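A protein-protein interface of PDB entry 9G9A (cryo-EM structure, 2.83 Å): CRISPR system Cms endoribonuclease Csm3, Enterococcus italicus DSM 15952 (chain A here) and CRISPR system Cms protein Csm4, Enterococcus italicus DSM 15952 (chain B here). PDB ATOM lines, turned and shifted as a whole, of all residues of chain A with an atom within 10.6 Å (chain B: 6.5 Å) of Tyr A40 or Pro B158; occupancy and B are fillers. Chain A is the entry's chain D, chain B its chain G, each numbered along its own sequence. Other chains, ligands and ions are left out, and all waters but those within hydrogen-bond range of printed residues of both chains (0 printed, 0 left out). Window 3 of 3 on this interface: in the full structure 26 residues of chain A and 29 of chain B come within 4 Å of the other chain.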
ATOM      1  N   VAL A  36     -37.495 -15.473   2.786  1.00  0.00           N
ATOM      2  CA  VAL A  36     -36.791 -14.290   2.309  1.00  0.00           C
ATOM      3  C   VAL A  36     -35.458 -14.715   1.708  1.00  0.00           C
ATOM      4  O   VAL A  36     -34.711 -15.504   2.300  1.00  0.00           O
ATOM      5  CB  VAL A  36     -36.612 -13.272   3.446  1.00  0.00           C
ATOM      6  CG1 VAL A  36     -35.980 -13.923   4.661  1.00  0.00           C
ATOM      7  CG2 VAL A  36     -35.782 -12.090   2.979  1.00  0.00           C
ATOM      8  N   ARG A  37     -35.162 -14.210   0.513  1.00  0.00           N
ATOM      9  CA  ARG A  37     -33.978 -14.605  -0.231  1.00  0.00           C
ATOM     10  C   ARG A  37     -33.237 -13.372  -0.719  1.00  0.00           C
ATOM     11  O   ARG A  37     -33.825 -12.300  -0.889  1.00  0.00           O
ATOM     12  CB  ARG A  37     -34.341 -15.495  -1.426  1.00  0.00           C
ATOM     13  CG  ARG A  37     -34.301 -16.981  -1.135  1.00  0.00           C
ATOM     14  CD  ARG A  37     -34.677 -17.784  -2.363  1.00  0.00           C
ATOM     15  NE  ARG A  37     -36.121 -17.882  -2.529  1.00  0.00           N
ATOM     16  CZ  ARG A  37     -36.830 -18.968  -2.252  1.00  0.00           C
ATOM     17  NH1 ARG A  37     -36.252 -20.076  -1.821  1.00  0.00           N
ATOM     18  NH2 ARG A  37     -38.149 -18.942  -2.418  1.00  0.00           N
ATOM     19  N   ASP A  38     -31.937 -13.534  -0.937  1.00  0.00           N
ATOM     20  CA  ASP A  38     -31.138 -12.456  -1.499  1.00  0.00           C
ATOM     21  C   ASP A  38     -31.587 -12.196  -2.934  1.00  0.00           C
ATOM     22  O   ASP A  38     -31.688 -13.143  -3.726  1.00  0.00           O
ATOM     23  CB  ASP A  38     -29.653 -12.812  -1.460  1.00  0.00           C
ATOM     24  CG  ASP A  38     -28.763 -11.646  -1.837  1.00  0.00           C
ATOM     25  OD1 ASP A  38     -28.824 -10.604  -1.148  1.00  0.00           O
ATOM     26  OD2 ASP A  38     -27.997 -11.769  -2.813  1.00  0.00           O
ATOM     27  N   PRO A  39     -31.885 -10.946  -3.302  1.00  0.00           N
ATOM     28  CA  PRO A  39     -32.420 -10.695  -4.650  1.00  0.00           C
ATOM     29  C   PRO A  39     -31.481 -11.109  -5.770  1.00  0.00           C
ATOM     30  O   PRO A  39     -31.947 -11.530  -6.837  1.00  0.00           O
ATOM     31  CB  PRO A  39     -32.672  -9.180  -4.645  1.00  0.00           C
ATOM     32  CG  PRO A  39     -31.767  -8.647  -3.588  1.00  0.00           C
ATOM     33  CD  PRO A  39     -31.717  -9.704  -2.531  1.00  0.00           C
ATOM     34  N   TYR A  40     -30.168 -11.003  -5.564  1.00  0.00           N
ATOM     35  CA  TYR A  40     -29.229 -11.345  -6.627  1.00  0.00           C
ATOM     36  C   TYR A  40     -28.974 -12.846  -6.684  1.00  0.00           C
ATOM     37  O   TYR A  40     -29.289 -13.501  -7.685  1.00  0.00           O
ATOM     38  CB  TYR A  40     -27.917 -10.586  -6.439  1.00  0.00           C
ATOM     39  CG  TYR A  40     -26.774 -11.147  -7.255  1.00  0.00           C
ATOM     40  CD1 TYR A  40     -26.775 -11.065  -8.640  1.00  0.00           C
ATOM     41  CD2 TYR A  40     -25.695 -11.764  -6.638  1.00  0.00           C
ATOM     42  CE1 TYR A  40     -25.734 -11.581  -9.388  1.00  0.00           C
ATOM     43  CE2 TYR A  40     -24.650 -12.283  -7.377  1.00  0.00           C
ATOM     44  CZ  TYR A  40     -24.673 -12.188  -8.752  1.00  0.00           C
ATOM     45  OH  TYR A  40     -23.634 -12.704  -9.491  1.00  0.00           O
ATOM     46  N   SER A  41     -28.414 -13.411  -5.616  1.00  0.00           N
ATOM     47  CA  SER A  41     -27.973 -14.800  -5.620  1.00  0.00           C
ATOM     48  C   SER A  41     -29.090 -15.794  -5.335  1.00  0.00           C
ATOM     49  O   SER A  41     -28.856 -17.003  -5.442  1.00  0.00           O
ATOM     50  CB  SER A  41     -26.845 -14.996  -4.601  1.00  0.00           C
ATOM     51  OG  SER A  41     -27.279 -14.678  -3.293  1.00  0.00           O
ATOM     52  N   ARG A  42     -30.286 -15.320  -4.979  1.00  0.00           N
ATOM     53  CA  ARG A  42     -31.433 -16.183  -4.690  1.00  0.00           C
ATOM     54  C   ARG A  42     -31.129 -17.154  -3.550  1.00  0.00           C
ATOM     55  O   ARG A  42     -31.681 -18.253  -3.482  1.00  0.00           O
ATOM     56  CB  ARG A  42     -31.892 -16.939  -5.940  1.00  0.00           C
ATOM     57  CG  ARG A  42     -32.624 -16.089  -6.969  1.00  0.00           C
ATOM     58  CD  ARG A  42     -34.027 -15.716  -6.502  1.00  0.00           C
ATOM     59  NE  ARG A  42     -34.048 -14.493  -5.707  1.00  0.00           N
ATOM     60  CZ  ARG A  42     -35.130 -13.998  -5.121  1.00  0.00           C
ATOM     61  NH1 ARG A  42     -36.301 -14.607  -5.206  1.00  0.00           N
ATOM     62  NH2 ARG A  42     -35.035 -12.867  -4.432  1.00  0.00           N
ATOM     63  N   LEU A  43     -30.243 -16.745  -2.648  1.00  0.00           N
ATOM     64  CA  LEU A  43     -29.906 -17.551  -1.491  1.00  0.00           C
ATOM     65  C   LEU A  43     -30.705 -17.092  -0.281  1.00  0.00           C
ATOM     66  O   LEU A  43     -30.953 -15.890  -0.124  1.00  0.00           O
ATOM     67  CB  LEU A  43     -28.410 -17.461  -1.166  1.00  0.00           C
ATOM     68  CG  LEU A  43     -27.442 -18.081  -2.173  1.00  0.00           C
ATOM     69  CD1 LEU A  43     -26.017 -17.953  -1.681  1.00  0.00           C
ATOM     70  CD2 LEU A  43     -27.794 -19.533  -2.417  1.00  0.00           C
ATOM     71  N   PRO A  44     -31.129 -18.014   0.583  1.00  0.00           N
ATOM     72  CA  PRO A  44     -31.863 -17.606   1.783  1.00  0.00           C
ATOM     73  C   PRO A  44     -31.001 -16.726   2.674  1.00  0.00           C
ATOM     74  O   PRO A  44     -29.782 -16.886   2.749  1.00  0.00           O
ATOM     75  CB  PRO A  44     -32.199 -18.937   2.466  1.00  0.00           C
ATOM     76  CG  PRO A  44     -32.101 -19.959   1.385  1.00  0.00           C
ATOM     77  CD  PRO A  44     -31.019 -19.477   0.473  1.00  0.00           C
ATOM     78  N   ILE A  45     -31.650 -15.773   3.340  1.00  0.00           N
ATOM     79  CA  ILE A  45     -30.978 -14.876   4.265  1.00  0.00           C
ATOM     80  C   ILE A  45     -31.789 -14.790   5.548  1.00  0.00           C
ATOM     81  O   ILE A  45     -32.987 -15.085   5.579  1.00  0.00           O
ATOM     82  CB  ILE A  45     -30.766 -13.463   3.681  1.00  0.00           C
ATOM     83  CG1 ILE A  45     -32.109 -12.820   3.333  1.00  0.00           C
ATOM     84  CG2 ILE A  45     -29.845 -13.508   2.473  1.00  0.00           C
ATOM     85  CD1 ILE A  45     -31.997 -11.388   2.871  1.00  0.00           C
ATOM     86  N   PHE A 102     -26.066 -14.123   5.900  1.00  0.00           N
ATOM     87  CA  PHE A 102     -26.003 -14.662   4.551  1.00  0.00           C
ATOM     88  C   PHE A 102     -25.700 -16.152   4.588  1.00  0.00           C
ATOM     89  O   PHE A 102     -24.917 -16.616   5.422  1.00  0.00           O
ATOM     90  CB  PHE A 102     -24.940 -13.932   3.728  1.00  0.00           C
ATOM     91  CG  PHE A 102     -25.138 -12.447   3.675  1.00  0.00           C
ATOM     92  CD1 PHE A 102     -26.073 -11.891   2.819  1.00  0.00           C
ATOM     93  CD2 PHE A 102     -24.394 -11.608   4.485  1.00  0.00           C
ATOM     94  CE1 PHE A 102     -26.261 -10.526   2.772  1.00  0.00           C
ATOM     95  CE2 PHE A 102     -24.578 -10.242   4.441  1.00  0.00           C
ATOM     96  CZ  PHE A 102     -25.512  -9.702   3.585  1.00  0.00           C
ATOM     97  N   GLN A 108     -23.094 -23.871   1.614  1.00  0.00           N
ATOM     98  CA  GLN A 108     -23.443 -23.898   0.199  1.00  0.00           C
ATOM     99  C   GLN A 108     -22.732 -25.042  -0.515  1.00  0.00           C
ATOM    100  O   GLN A 108     -23.342 -25.773  -1.302  1.00  0.00           O
ATOM    101  CB  GLN A 108     -23.099 -22.551  -0.439  1.00  0.00           C
ATOM    102  CG  GLN A 108     -23.675 -22.341  -1.823  1.00  0.00           C
ATOM    103  CD  GLN A 108     -23.558 -20.902  -2.283  1.00  0.00           C
ATOM    104  OE1 GLN A 108     -23.229 -20.013  -1.499  1.00  0.00           O
ATOM    105  NE2 GLN A 108     -23.828 -20.665  -3.561  1.00  0.00           N
ATOM    106  N   THR B  12     -17.130  -1.346  -1.399  1.00  0.00           N
ATOM    107  CA  THR B  12     -17.713  -2.641  -1.720  1.00  0.00           C
ATOM    108  C   THR B  12     -18.674  -3.019  -0.604  1.00  0.00           C
ATOM    109  O   THR B  12     -18.277  -3.088   0.562  1.00  0.00           O
ATOM    110  CB  THR B  12     -16.632  -3.714  -1.868  1.00  0.00           C
ATOM    111  OG1 THR B  12     -15.643  -3.274  -2.806  1.00  0.00           O
ATOM    112  CG2 THR B  12     -17.239  -5.017  -2.357  1.00  0.00           C
ATOM    113  N   LYS B  68     -17.018  -4.535 -12.741  1.00  0.00           N
ATOM    114  CA  LYS B  68     -15.768  -5.210 -13.065  1.00  0.00           C
ATOM    115  C   LYS B  68     -15.104  -4.643 -14.313  1.00  0.00           C
ATOM    116  O   LYS B  68     -13.914  -4.887 -14.529  1.00  0.00           O
ATOM    117  CB  LYS B  68     -16.014  -6.708 -13.247  1.00  0.00           C
ATOM    118  CG  LYS B  68     -16.959  -7.053 -14.384  1.00  0.00           C
ATOM    119  CD  LYS B  68     -17.225  -8.546 -14.444  1.00  0.00           C
ATOM    120  CE  LYS B  68     -17.956  -9.018 -13.199  1.00  0.00           C
ATOM    121  NZ  LYS B  68     -18.209 -10.485 -13.221  1.00  0.00           N
ATOM    122  N   ASN B 125     -23.812  -2.484 -14.761  1.00  0.00           N
ATOM    123  CA  ASN B 125     -23.857  -3.751 -14.040  1.00  0.00           C
ATOM    124  C   ASN B 125     -23.750  -3.503 -12.543  1.00  0.00           C
ATOM    125  O   ASN B 125     -22.972  -4.140 -11.829  1.00  0.00           O
ATOM    126  CB  ASN B 125     -22.749  -4.677 -14.538  1.00  0.00           C
ATOM    127  CG  ASN B 125     -23.042  -6.140 -14.268  1.00  0.00           C
ATOM    128  OD1 ASN B 125     -23.921  -6.735 -14.894  1.00  0.00           O
ATOM    129  ND2 ASN B 125     -22.294  -6.734 -13.346  1.00  0.00           N
ATOM    130  N   LEU B 126     -24.544  -2.552 -12.048  1.00  0.00           N
ATOM    131  CA  LEU B 126     -24.467  -2.172 -10.641  1.00  0.00           C
ATOM    132  C   LEU B 126     -25.022  -3.266  -9.741  1.00  0.00           C
ATOM    133  O   LEU B 126     -24.304  -3.829  -8.906  1.00  0.00           O
ATOM    134  CB  LEU B 126     -25.222  -0.865 -10.411  1.00  0.00           C
ATOM    135  CG  LEU B 126     -24.405   0.308  -9.877  1.00  0.00           C
ATOM    136  CD1 LEU B 126     -25.312   1.333  -9.223  1.00  0.00           C
ATOM    137  CD2 LEU B 126     -23.323  -0.153  -8.917  1.00  0.00           C
ATOM    138  N   LYS B 128     -29.145  -5.040  -8.211  1.00  0.00           N
ATOM    139  CA  LYS B 128     -30.590  -5.198  -8.283  1.00  0.00           C
ATOM    140  C   LYS B 128     -31.249  -4.502  -7.102  1.00  0.00           C
ATOM    141  O   LYS B 128     -30.844  -4.699  -5.953  1.00  0.00           O
ATOM    142  CB  LYS B 128     -30.983  -6.678  -8.307  1.00  0.00           C
ATOM    143  CG  LYS B 128     -32.469  -6.914  -8.510  1.00  0.00           C
ATOM    144  CD  LYS B 128     -32.779  -8.388  -8.685  1.00  0.00           C
ATOM    145  CE  LYS B 128     -34.270  -8.618  -8.855  1.00  0.00           C
ATOM    146  NZ  LYS B 128     -34.813  -7.882 -10.028  1.00  0.00           N
ATOM    147  N   THR B 155     -28.971  -4.349  -3.764  1.00  0.00           N
ATOM    148  CA  THR B 155     -27.892  -5.315  -3.614  1.00  0.00           C
ATOM    149  C   THR B 155     -26.956  -5.192  -4.809  1.00  0.00           C
ATOM    150  O   THR B 155     -27.367  -5.429  -5.950  1.00  0.00           O
ATOM    151  CB  THR B 155     -28.437  -6.739  -3.509  1.00  0.00           C
ATOM    152  OG1 THR B 155     -29.340  -6.825  -2.400  1.00  0.00           O
ATOM    153  CG2 THR B 155     -27.301  -7.733  -3.311  1.00  0.00           C
ATOM    154  N   PHE B 156     -25.710  -4.816  -4.544  1.00  0.00           N
ATOM    155  CA  PHE B 156     -24.728  -4.655  -5.604  1.00  0.00           C
ATOM    156  C   PHE B 156     -24.229  -6.011  -6.092  1.00  0.00           C
ATOM    157  O   PHE B 156     -24.240  -7.006  -5.362  1.00  0.00           O
ATOM    158  CB  PHE B 156     -23.551  -3.812  -5.116  1.00  0.00           C
ATOM    159  CG  PHE B 156     -23.919  -2.396  -4.780  1.00  0.00           C
ATOM    160  CD1 PHE B 156     -24.376  -2.065  -3.519  1.00  0.00           C
ATOM    161  CD2 PHE B 156     -23.803  -1.398  -5.727  1.00  0.00           C
ATOM    162  CE1 PHE B 156     -24.711  -0.765  -3.212  1.00  0.00           C
ATOM    163  CE2 PHE B 156     -24.137  -0.097  -5.424  1.00  0.00           C
ATOM    164  CZ  PHE B 156     -24.591   0.219  -4.166  1.00  0.00           C
ATOM    165  N   TYR B 157     -23.790  -6.041  -7.346  1.00  0.00           N
ATOM    166  CA  TYR B 157     -23.229  -7.249  -7.918  1.00  0.00           C
ATOM    167  C   TYR B 157     -21.848  -7.517  -7.319  1.00  0.00           C
ATOM    168  O   TYR B 157     -21.213  -6.609  -6.777  1.00  0.00           O
ATOM    169  CB  TYR B 157     -23.166  -7.121  -9.438  1.00  0.00           C
ATOM    170  CG  TYR B 157     -24.523  -7.242 -10.099  1.00  0.00           C
ATOM    171  CD1 TYR B 157     -25.585  -7.844  -9.441  1.00  0.00           C
ATOM    172  CD2 TYR B 157     -24.742  -6.755 -11.378  1.00  0.00           C
ATOM    173  CE1 TYR B 157     -26.826  -7.958 -10.038  1.00  0.00           C
ATOM    174  CE2 TYR B 157     -25.980  -6.866 -11.983  1.00  0.00           C
ATOM    175  CZ  TYR B 157     -27.019  -7.467 -11.309  1.00  0.00           C
ATOM    176  OH  TYR B 157     -28.254  -7.579 -11.905  1.00  0.00           O
ATOM    177  N   PRO B 158     -21.372  -8.767  -7.384  1.00  0.00           N
ATOM    178  CA  PRO B 158     -20.148  -9.117  -6.639  1.00  0.00           C
ATOM    179  C   PRO B 158     -18.938  -8.265  -6.985  1.00  0.00           C
ATOM    180  O   PRO B 158     -18.149  -7.937  -6.091  1.00  0.00           O
ATOM    181  CB  PRO B 158     -19.931 -10.589  -7.011  1.00  0.00           C
ATOM    182  CG  PRO B 158     -21.287 -11.094  -7.325  1.00  0.00           C
ATOM    183  CD  PRO B 158     -22.001  -9.957  -7.987  1.00  0.00           C
ATOM    184  N   GLU B 159     -18.765  -7.895  -8.250  1.00  0.00           N
ATOM    185  CA  GLU B 159     -17.629  -7.085  -8.667  1.00  0.00           C
ATOM    186  C   GLU B 159     -17.979  -5.612  -8.821  1.00  0.00           C
ATOM    187  O   GLU B 159     -17.123  -4.821  -9.230  1.00  0.00           O
ATOM    188  CB  GLU B 159     -17.050  -7.625  -9.975  1.00  0.00           C
ATOM    189  CG  GLU B 159     -16.328  -8.959  -9.844  1.00  0.00           C
ATOM    190  CD  GLU B 159     -14.950  -8.827  -9.223  1.00  0.00           C
ATOM    191  OE1 GLU B 159     -14.496  -7.685  -9.007  1.00  0.00           O
ATOM    192  OE2 GLU B 159     -14.317  -9.869  -8.953  1.00  0.00           O
ATOM    193  N   SER B 160     -19.211  -5.226  -8.507  1.00  0.00           N
ATOM    194  CA  SER B 160     -19.647  -3.845  -8.632  1.00  0.00           C
ATOM    195  C   SER B 160     -19.502  -3.133  -7.287  1.00  0.00           C
ATOM    196  O   SER B 160     -18.979  -3.686  -6.316  1.00  0.00           O
ATOM    197  CB  SER B 160     -21.081  -3.792  -9.150  1.00  0.00           C
ATOM    198  OG  SER B 160     -21.174  -4.374 -10.438  1.00  0.00           O
ATOM    199  N   GLY B 161     -19.968  -1.894  -7.220  1.00  0.00           N
ATOM    200  CA  GLY B 161     -19.874  -1.118  -6.002  1.00  0.00           C
ATOM    201  C   GLY B 161     -19.949   0.363  -6.319  1.00  0.00           C
ATOM    202  O   GLY B 161     -20.288   0.762  -7.433  1.00  0.00           O
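OD2 of Asp A38 sits at hydrogen-bond distance from OG of Ser A41, at 3.0 Å. The backbone carbonyl oxygen (O) of Asp A38 lies close to the guanidinium group (NE) of Arg A42, 3.4 Å away. N of Asp A38 lies within hydrogen-bond range of O of Leu A43 (2.7 Å). O of Leu B126 lies within hydrogen-bond range of N of Tyr B157, at 2.8 Å. N of Thr B155 lies within hydrogen-bond range of O of Lys B128 (2.9 Å).
Asp A38 touches Thr B155 (OD1 to CG2, 3.9 Å). Pro A39 touches Lys B128 (O to CD, 3.7 Å). Thr B155 touches Pro A39. CE1 of Tyr B157 touches CD1 of Tyr A40, at 3.4 Å. Pro B158 touches Tyr A40.
Of the printed residues of chain B, Tyr A40 touches Tyr B157 and Pro B158. No residue of chain A comes within 4 Å of Glu B159. No residue of chain A comes within 4 Å of Ser B160. Of the printed residues of chain A, Lys B128 touches Pro A39. Of the printed residues of chain B, Asp A38 touches Thr B155 (3.9 Å). Printed residues of chain A within 4 Å of Thr B155: Asp A38 and Pro A39. Of the printed residues of chain B, Pro A39 touches Lys B128 (3.7 Å) and Thr B155 (3.3 Å). Arg A37 touches none of the printed residues of chain B. Leu A43 touches none of the printed residues of chain B. The nearest residue of chain A that does not touch Pro B158 is Ser A41 (7.3 Å). The nearest printed residue of chain B that does not touch Pro A39 is Tyr B157 (7.0 Å).
Along chain A the printed residues that touch a printed residue of chain B span positions 38 to 40. Printed residues of chain B that touch a printed residue of chain A: Lys B128, Thr B155, Tyr B157 and Pro B158. Among the printed residues, 5 pairs touch across the chains.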
